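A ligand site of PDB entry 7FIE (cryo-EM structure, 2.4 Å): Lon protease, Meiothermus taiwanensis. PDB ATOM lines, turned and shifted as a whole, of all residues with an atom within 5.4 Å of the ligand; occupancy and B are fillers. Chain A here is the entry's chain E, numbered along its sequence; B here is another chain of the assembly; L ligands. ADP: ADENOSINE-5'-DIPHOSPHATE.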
ATOM      1  N   ASP A 318       3.241  16.531  14.261  1.00  0.00           N
ATOM      2  CA  ASP A 318       3.143  17.825  14.913  1.00  0.00           C
ATOM      3  C   ASP A 318       3.070  18.995  13.951  1.00  0.00           C
ATOM      4  O   ASP A 318       2.612  20.070  14.351  1.00  0.00           O
ATOM      5  CB  ASP A 318       4.350  18.039  15.840  1.00  0.00           C
ATOM      6  CG  ASP A 318       4.388  17.057  16.971  1.00  0.00           C
ATOM      7  OD1 ASP A 318       3.305  16.563  17.358  1.00  0.00           O
ATOM      8  OD2 ASP A 318       5.489  16.767  17.477  1.00  0.00           O
ATOM      9  N   HIS A 319       3.500  18.822  12.710  1.00  0.00           N
ATOM     10  CA  HIS A 319       3.660  19.945  11.798  1.00  0.00           C
ATOM     11  C   HIS A 319       3.012  19.614  10.471  1.00  0.00           C
ATOM     12  O   HIS A 319       2.329  18.593  10.319  1.00  0.00           O
ATOM     13  CB  HIS A 319       5.133  20.296  11.607  1.00  0.00           C
ATOM     14  CG  HIS A 319       5.787  20.790  12.855  1.00  0.00           C
ATOM     15  ND1 HIS A 319       6.363  19.930  13.774  1.00  0.00           N
ATOM     16  CD2 HIS A 319       5.954  22.032  13.345  1.00  0.00           C
ATOM     17  CE1 HIS A 319       6.857  20.643  14.773  1.00  0.00           C
ATOM     18  NE2 HIS A 319       6.620  21.922  14.542  1.00  0.00           N
ATOM     19  N   TYR A 320       3.227  20.499   9.499  1.00  0.00           N
ATOM     20  CA  TYR A 320       2.615  20.354   8.184  1.00  0.00           C
ATOM     21  C   TYR A 320       3.625  20.782   7.130  1.00  0.00           C
ATOM     22  O   TYR A 320       4.010  21.951   7.084  1.00  0.00           O
ATOM     23  CB  TYR A 320       1.352  21.201   8.072  1.00  0.00           C
ATOM     24  CG  TYR A 320       0.659  21.049   6.738  1.00  0.00           C
ATOM     25  CD1 TYR A 320      -0.115  19.937   6.473  1.00  0.00           C
ATOM     26  CD2 TYR A 320       0.787  22.013   5.757  1.00  0.00           C
ATOM     27  CE1 TYR A 320      -0.753  19.791   5.258  1.00  0.00           C
ATOM     28  CE2 TYR A 320       0.160  21.868   4.533  1.00  0.00           C
ATOM     29  CZ  TYR A 320      -0.604  20.755   4.290  1.00  0.00           C
ATOM     30  OH  TYR A 320      -1.233  20.614   3.086  1.00  0.00           O
ATOM     31  N   GLY A 321       4.033  19.840   6.287  1.00  0.00           N
ATOM     32  CA  GLY A 321       5.049  20.137   5.297  1.00  0.00           C
ATOM     33  C   GLY A 321       6.434  19.967   5.893  1.00  0.00           C
ATOM     34  O   GLY A 321       6.732  18.995   6.587  1.00  0.00           O
ATOM     35  N   LEU A 322       7.295  20.959   5.597  1.00  0.00           N
ATOM     36  CA  LEU A 322       8.608  21.153   6.221  1.00  0.00           C
ATOM     37  C   LEU A 322       9.560  19.974   6.011  1.00  0.00           C
ATOM     38  O   LEU A 322      10.022  19.374   6.978  1.00  0.00           O
ATOM     39  CB  LEU A 322       8.473  21.410   7.728  1.00  0.00           C
ATOM     40  CG  LEU A 322       8.233  22.806   8.275  1.00  0.00           C
ATOM     41  CD1 LEU A 322       9.368  23.709   7.869  1.00  0.00           C
ATOM     42  CD2 LEU A 322       6.902  23.384   7.847  1.00  0.00           C
ATOM     43  N   PRO A 356      11.534  33.746   9.084  1.00  0.00           N
ATOM     44  CA  PRO A 356      10.660  34.786   9.648  1.00  0.00           C
ATOM     45  C   PRO A 356      10.100  34.344  10.989  1.00  0.00           C
ATOM     46  O   PRO A 356      10.022  33.133  11.258  1.00  0.00           O
ATOM     47  CB  PRO A 356       9.553  34.911   8.589  1.00  0.00           C
ATOM     48  CG  PRO A 356      10.178  34.416   7.336  1.00  0.00           C
ATOM     49  CD  PRO A 356      11.075  33.311   7.763  1.00  0.00           C
ATOM     50  N   PRO A 357       9.695  35.275  11.865  1.00  0.00           N
ATOM     51  CA  PRO A 357       9.364  34.901  13.250  1.00  0.00           C
ATOM     52  C   PRO A 357       8.081  34.106  13.425  1.00  0.00           C
ATOM     53  O   PRO A 357       7.958  33.395  14.419  1.00  0.00           O
ATOM     54  CB  PRO A 357       9.254  36.258  13.947  1.00  0.00           C
ATOM     55  CG  PRO A 357       8.862  37.188  12.889  1.00  0.00           C
ATOM     56  CD  PRO A 357       9.579  36.729  11.669  1.00  0.00           C
ATOM     57  N   GLY A 358       7.135  34.197  12.499  1.00  0.00           N
ATOM     58  CA  GLY A 358       5.894  33.471  12.684  1.00  0.00           C
ATOM     59  C   GLY A 358       5.998  32.005  12.343  1.00  0.00           C
ATOM     60  O   GLY A 358       5.148  31.202  12.730  1.00  0.00           O
ATOM     61  N   VAL A 359       7.039  31.643  11.596  1.00  0.00           N
ATOM     62  CA  VAL A 359       7.270  30.239  11.266  1.00  0.00           C
ATOM     63  C   VAL A 359       7.854  29.542  12.490  1.00  0.00           C
ATOM     64  O   VAL A 359       8.722  30.076  13.184  1.00  0.00           O
ATOM     65  CB  VAL A 359       8.195  30.124  10.052  1.00  0.00           C
ATOM     66  CG1 VAL A 359       8.259  28.708   9.581  1.00  0.00           C
ATOM     67  CG2 VAL A 359       7.737  31.040   8.937  1.00  0.00           C
ATOM     68  N   GLY A 360       7.407  28.308  12.719  1.00  0.00           N
ATOM     69  CA  GLY A 360       7.511  27.661  14.015  1.00  0.00           C
ATOM     70  C   GLY A 360       8.855  27.079  14.415  1.00  0.00           C
ATOM     71  O   GLY A 360       9.078  25.878  14.243  1.00  0.00           O
ATOM     72  N   LYS A 361       9.755  27.910  14.939  1.00  0.00           N
ATOM     73  CA  LYS A 361      11.071  27.386  15.342  1.00  0.00           C
ATOM     74  C   LYS A 361      10.971  26.554  16.616  1.00  0.00           C
ATOM     75  O   LYS A 361      11.414  25.389  16.650  1.00  0.00           O
ATOM     76  CB  LYS A 361      12.058  28.525  15.597  1.00  0.00           C
ATOM     77  CG  LYS A 361      12.859  29.039  14.413  1.00  0.00           C
ATOM     78  CD  LYS A 361      12.018  29.816  13.439  1.00  0.00           C
ATOM     79  CE  LYS A 361      12.871  30.355  12.329  1.00  0.00           C
ATOM     80  NZ  LYS A 361      13.875  31.290  12.883  1.00  0.00           N
ATOM     81  N   THR A 362      10.414  27.133  17.672  1.00  0.00           N
ATOM     82  CA  THR A 362      10.408  26.465  18.970  1.00  0.00           C
ATOM     83  C   THR A 362       9.478  25.269  18.995  1.00  0.00           C
ATOM     84  O   THR A 362       9.651  24.373  19.822  1.00  0.00           O
ATOM     85  CB  THR A 362      10.038  27.448  20.077  1.00  0.00           C
ATOM     86  OG1 THR A 362       8.727  27.964  19.832  1.00  0.00           O
ATOM     87  CG2 THR A 362      11.024  28.591  20.113  1.00  0.00           C
ATOM     88  N   SER A 363       8.492  25.216  18.099  1.00  0.00           N
ATOM     89  CA  SER A 363       7.678  24.003  17.977  1.00  0.00           C
ATOM     90  C   SER A 363       8.512  22.852  17.444  1.00  0.00           C
ATOM     91  O   SER A 363       8.387  21.721  17.937  1.00  0.00           O
ATOM     92  CB  SER A 363       6.472  24.252  17.083  1.00  0.00           C
ATOM     93  OG  SER A 363       6.879  24.477  15.744  1.00  0.00           O
ATOM     94  N   ASP A 422      17.404  31.396  21.447  1.00  0.00           N
ATOM     95  CA  ASP A 422      16.542  32.186  20.581  1.00  0.00           C
ATOM     96  C   ASP A 422      17.127  33.582  20.362  1.00  0.00           C
ATOM     97  O   ASP A 422      17.644  34.197  21.294  1.00  0.00           O
ATOM     98  CB  ASP A 422      15.142  32.276  21.194  1.00  0.00           C
ATOM     99  CG  ASP A 422      14.142  32.946  20.277  1.00  0.00           C
ATOM    100  OD1 ASP A 422      13.754  32.334  19.257  1.00  0.00           O
ATOM    101  OD2 ASP A 422      13.715  34.073  20.597  1.00  0.00           O
ATOM    102  N   TYR A 493       5.386  30.358   4.448  1.00  0.00           N
ATOM    103  CA  TYR A 493       4.263  29.597   3.951  1.00  0.00           C
ATOM    104  C   TYR A 493       3.489  30.373   2.903  1.00  0.00           C
ATOM    105  O   TYR A 493       3.487  31.599   2.889  1.00  0.00           O
ATOM    106  CB  TYR A 493       3.310  29.208   5.086  1.00  0.00           C
ATOM    107  CG  TYR A 493       3.956  28.402   6.167  1.00  0.00           C
ATOM    108  CD1 TYR A 493       4.195  27.047   6.003  1.00  0.00           C
ATOM    109  CD2 TYR A 493       4.330  28.995   7.366  1.00  0.00           C
ATOM    110  CE1 TYR A 493       4.791  26.312   6.998  1.00  0.00           C
ATOM    111  CE2 TYR A 493       4.914  28.266   8.359  1.00  0.00           C
ATOM    112  CZ  TYR A 493       5.151  26.925   8.170  1.00  0.00           C
ATOM    113  OH  TYR A 493       5.739  26.213   9.180  1.00  0.00           O
ATOM    114  N   ILE A 501      -2.642  24.770   8.007  1.00  0.00           N
ATOM    115  CA  ILE A 501      -2.165  24.901   9.381  1.00  0.00           C
ATOM    116  C   ILE A 501      -3.275  25.427  10.287  1.00  0.00           C
ATOM    117  O   ILE A 501      -3.460  24.960  11.412  1.00  0.00           O
ATOM    118  CB  ILE A 501      -0.912  25.789   9.418  1.00  0.00           C
ATOM    119  CG1 ILE A 501       0.274  25.077   8.772  1.00  0.00           C
ATOM    120  CG2 ILE A 501      -0.532  26.161  10.826  1.00  0.00           C
ATOM    121  CD1 ILE A 501       1.441  25.992   8.491  1.00  0.00           C
ATOM    122  N   TYR A 505      -4.272  22.455  12.976  1.00  0.00           N
ATOM    123  CA  TYR A 505      -3.502  22.546  14.200  1.00  0.00           C
ATOM    124  C   TYR A 505      -3.845  23.750  15.061  1.00  0.00           C
ATOM    125  O   TYR A 505      -3.875  23.647  16.283  1.00  0.00           O
ATOM    126  CB  TYR A 505      -2.012  22.560  13.864  1.00  0.00           C
ATOM    127  CG  TYR A 505      -1.505  21.251  13.308  1.00  0.00           C
ATOM    128  CD1 TYR A 505      -1.142  20.210  14.151  1.00  0.00           C
ATOM    129  CD2 TYR A 505      -1.416  21.050  11.938  1.00  0.00           C
ATOM    130  CE1 TYR A 505      -0.684  19.019  13.644  1.00  0.00           C
ATOM    131  CE2 TYR A 505      -0.959  19.859  11.431  1.00  0.00           C
ATOM    132  CZ  TYR A 505      -0.595  18.851  12.276  1.00  0.00           C
ATOM    133  OH  TYR A 505      -0.137  17.657  11.759  1.00  0.00           O
ATOM    134  N   LEU A 506      -4.118  24.901  14.441  1.00  0.00           N
ATOM    135  CA  LEU A 506      -4.266  26.135  15.204  1.00  0.00           C
ATOM    136  C   LEU A 506      -5.657  26.263  15.829  1.00  0.00           C
ATOM    137  O   LEU A 506      -5.783  26.506  17.040  1.00  0.00           O
ATOM    138  CB  LEU A 506      -3.986  27.341  14.309  1.00  0.00           C
ATOM    139  CG  LEU A 506      -2.558  27.487  13.778  1.00  0.00           C
ATOM    140  CD1 LEU A 506      -2.500  28.669  12.840  1.00  0.00           C
ATOM    141  CD2 LEU A 506      -1.584  27.678  14.910  1.00  0.00           C
ATOM    142  N   LYS A 509      -6.547  23.799  18.876  1.00  0.00           N
ATOM    143  CA  LYS A 509      -5.901  24.113  20.145  1.00  0.00           C
ATOM    144  C   LYS A 509      -6.383  25.443  20.710  1.00  0.00           C
ATOM    145  O   LYS A 509      -6.508  25.582  21.935  1.00  0.00           O
ATOM    146  CB  LYS A 509      -4.374  24.078  20.022  1.00  0.00           C
ATOM    147  CG  LYS A 509      -3.726  25.165  19.201  1.00  0.00           C
ATOM    148  CD  LYS A 509      -2.224  24.962  19.125  1.00  0.00           C
ATOM    149  CE  LYS A 509      -1.554  26.046  18.308  1.00  0.00           C
ATOM    150  NZ  LYS A 509      -0.085  25.851  18.216  1.00  0.00           N
ATOM    151  N   VAL A 540       2.597  32.497  10.891  1.00  0.00           N
ATOM    152  CA  VAL A 540       1.226  32.189  11.281  1.00  0.00           C
ATOM    153  C   VAL A 540       0.929  32.684  12.689  1.00  0.00           C
ATOM    154  O   VAL A 540       0.029  32.162  13.365  1.00  0.00           O
ATOM    155  CB  VAL A 540       0.954  30.684  11.162  1.00  0.00           C
ATOM    156  CG1 VAL A 540       0.931  30.247   9.720  1.00  0.00           C
ATOM    157  CG2 VAL A 540       2.035  29.919  11.883  1.00  0.00           C
ATOM    158  N   ARG A 541       1.671  33.699  13.150  1.00  0.00           N
ATOM    159  CA  ARG A 541       1.503  34.187  14.514  1.00  0.00           C
ATOM    160  C   ARG A 541       0.284  35.092  14.643  1.00  0.00           C
ATOM    161  O   ARG A 541      -0.517  34.953  15.582  1.00  0.00           O
ATOM    162  CB  ARG A 541       2.769  34.938  14.937  1.00  0.00           C
ATOM    163  CG  ARG A 541       2.743  35.433  16.369  1.00  0.00           C
ATOM    164  CD  ARG A 541       2.780  34.275  17.334  1.00  0.00           C
ATOM    165  NE  ARG A 541       2.817  34.711  18.716  1.00  0.00           N
ATOM    166  CZ  ARG A 541       2.715  33.890  19.759  1.00  0.00           C
ATOM    167  NH1 ARG A 541       2.570  32.595  19.564  1.00  0.00           N
ATOM    168  NH2 ARG A 541       2.764  34.375  20.996  1.00  0.00           N
ATOM    169  N   GLU A 544      -2.832  33.132  14.476  1.00  0.00           N
ATOM    170  CA  GLU A 544      -3.076  32.525  15.782  1.00  0.00           C
ATOM    171  C   GLU A 544      -3.780  33.494  16.726  1.00  0.00           C
ATOM    172  O   GLU A 544      -4.739  33.129  17.408  1.00  0.00           O
ATOM    173  CB  GLU A 544      -1.761  32.070  16.396  1.00  0.00           C
ATOM    174  CG  GLU A 544      -1.901  31.483  17.782  1.00  0.00           C
ATOM    175  CD  GLU A 544      -0.570  31.177  18.415  1.00  0.00           C
ATOM    176  OE1 GLU A 544       0.468  31.448  17.775  1.00  0.00           O
ATOM    177  OE2 GLU A 544      -0.547  30.681  19.561  1.00  0.00           O
ATOM    178  N   ARG B 479      11.315  40.014  26.521  1.00  0.00           N
ATOM    179  CA  ARG B 479      10.803  39.167  25.448  1.00  0.00           C
ATOM    180  C   ARG B 479      10.103  37.871  25.878  1.00  0.00           C
ATOM    181  O   ARG B 479       9.068  37.552  25.287  1.00  0.00           O
ATOM    182  CB  ARG B 479      11.949  38.877  24.459  1.00  0.00           C
ATOM    183  CG  ARG B 479      11.607  37.970  23.297  1.00  0.00           C
ATOM    184  CD  ARG B 479      10.568  38.598  22.386  1.00  0.00           C
ATOM    185  NE  ARG B 479      10.318  37.767  21.207  1.00  0.00           N
ATOM    186  CZ  ARG B 479       9.474  36.742  21.171  1.00  0.00           C
ATOM    187  NH1 ARG B 479       8.791  36.404  22.244  1.00  0.00           N
ATOM    188  NH2 ARG B 479       9.325  36.052  20.043  1.00  0.00           N
HETATM  189  PB  ADP L   1       8.821  31.042  16.539  1.00  0.00           P
HETATM  190  O1B ADP L   1       8.725  32.212  17.480  1.00  0.00           O
HETATM  191  O2B ADP L   1       9.355  29.818  17.199  1.00  0.00           O
HETATM  192  O3B ADP L   1       9.554  31.380  15.296  1.00  0.00           O
HETATM  193  PA  ADP L   1       6.278  29.920  17.112  1.00  0.00           P
HETATM  194  O1A ADP L   1       6.420  30.491  18.485  1.00  0.00           O
HETATM  195  O2A ADP L   1       6.460  28.448  16.938  1.00  0.00           O
HETATM  196  O3A ADP L   1       7.308  30.673  16.159  1.00  0.00           O
HETATM  197  O5' ADP L   1       4.864  30.353  16.522  1.00  0.00           O
HETATM  198  C5' ADP L   1       4.362  29.578  15.423  1.00  0.00           C
HETATM  199  C4' ADP L   1       2.994  29.066  15.779  1.00  0.00           C
HETATM  200  O4' ADP L   1       2.477  28.349  14.633  1.00  0.00           O
HETATM  201  C3' ADP L   1       2.945  28.024  16.903  1.00  0.00           C
HETATM  202  O3' ADP L   1       1.606  27.878  17.341  1.00  0.00           O
HETATM  203  C2' ADP L   1       3.341  26.772  16.122  1.00  0.00           C
HETATM  204  O2' ADP L   1       3.038  25.574  16.796  1.00  0.00           O
HETATM  205  C1' ADP L   1       2.486  26.961  14.873  1.00  0.00           C
HETATM  206  N9  ADP L   1       3.051  26.309  13.701  1.00  0.00           N
HETATM  207  C8  ADP L   1       4.159  26.702  12.999  1.00  0.00           C
HETATM  208  N7  ADP L   1       4.431  25.921  11.987  1.00  0.00           N
HETATM  209  C5  ADP L   1       3.424  24.970  12.007  1.00  0.00           C
HETATM  210  C6  ADP L   1       3.156  23.875  11.179  1.00  0.00           C
HETATM  211  N6  ADP L   1       3.900  23.536  10.130  1.00  0.00           N
HETATM  212  N1  ADP L   1       2.063  23.125  11.471  1.00  0.00           N
HETATM  213  C2  ADP L   1       1.324  23.479  12.527  1.00  0.00           C
HETATM  214  N3  ADP L   1       1.474  24.480  13.373  1.00  0.00           N
HETATM  215  C4  ADP L   1       2.567  25.201  13.057  1.00  0.00           C
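The side-chain carboxylate (OE1) of Glu 544 lies within salt-bridge range of the guanidinium group (NH1) of Arg 541 (3.0 Å). The backbone carbonyl oxygen (O) of His 319 sits at hydrogen-bond distance from the side-chain hydroxyl (OH) of Tyr 505. The backbone NH of Leu 506 is in hydrogen-bond range of the backbone carbonyl oxygen of Ile 501, at 3.1 Å. The backbone carbonyl oxygen (O) of Gly 360 is in hydrogen-bond range of the side-chain hydroxyl (OG) of Ser 363 (3.0 Å). The backbone NH (N) of Val 540 lies within hydrogen-bond range of the backbone carbonyl oxygen (O) of Gly 358, at 3.4 Å. NE2 of His 319 sits at hydrogen-bond distance from OG of Ser 363 (2.8 Å).
Merely in contact with the ligand: Val 540 (3.2 Å), Gly 360 (3.2 Å), Gly 358 (3.2 Å), His 319 (3.6 Å), Ile 501 (3.7 Å), Tyr 505 (3.7 Å), Ser 363 (3.7 Å), Glu 544 (3.8 Å) and Leu 322 (3.8 Å).
The backbone NH of Thr 362 lies within hydrogen-bond range of an oxygen (O2B) of the ligand (2.9 Å). An oxygen (O3B) of the ligand sits close to the backbone carbonyl oxygen (O) of Val 359, 2.6 Å away. N6 of the ligand lies within hydrogen-bond range of O of Tyr 320 (3.4 Å). OH of Tyr 493 lies within hydrogen-bond range of N7 of the ligand (3.1 Å). An oxygen (O3') of the ligand lies within hydrogen-bond range of the side-chain amino group (NZ) of Lys 509. A nitrogen (N1) of the ligand is in hydrogen-bond range of the backbone NH (N) of Tyr 320 (3.5 Å). O3B of the ligand sits close to O of Pro 357 (2.7 Å). N of Lys 361 lies within hydrogen-bond range of O2B of the ligand, 3.0 Å away. OG1 of Thr 362 sits at hydrogen-bond distance from O2B of the ligand, 3.3 Å away.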
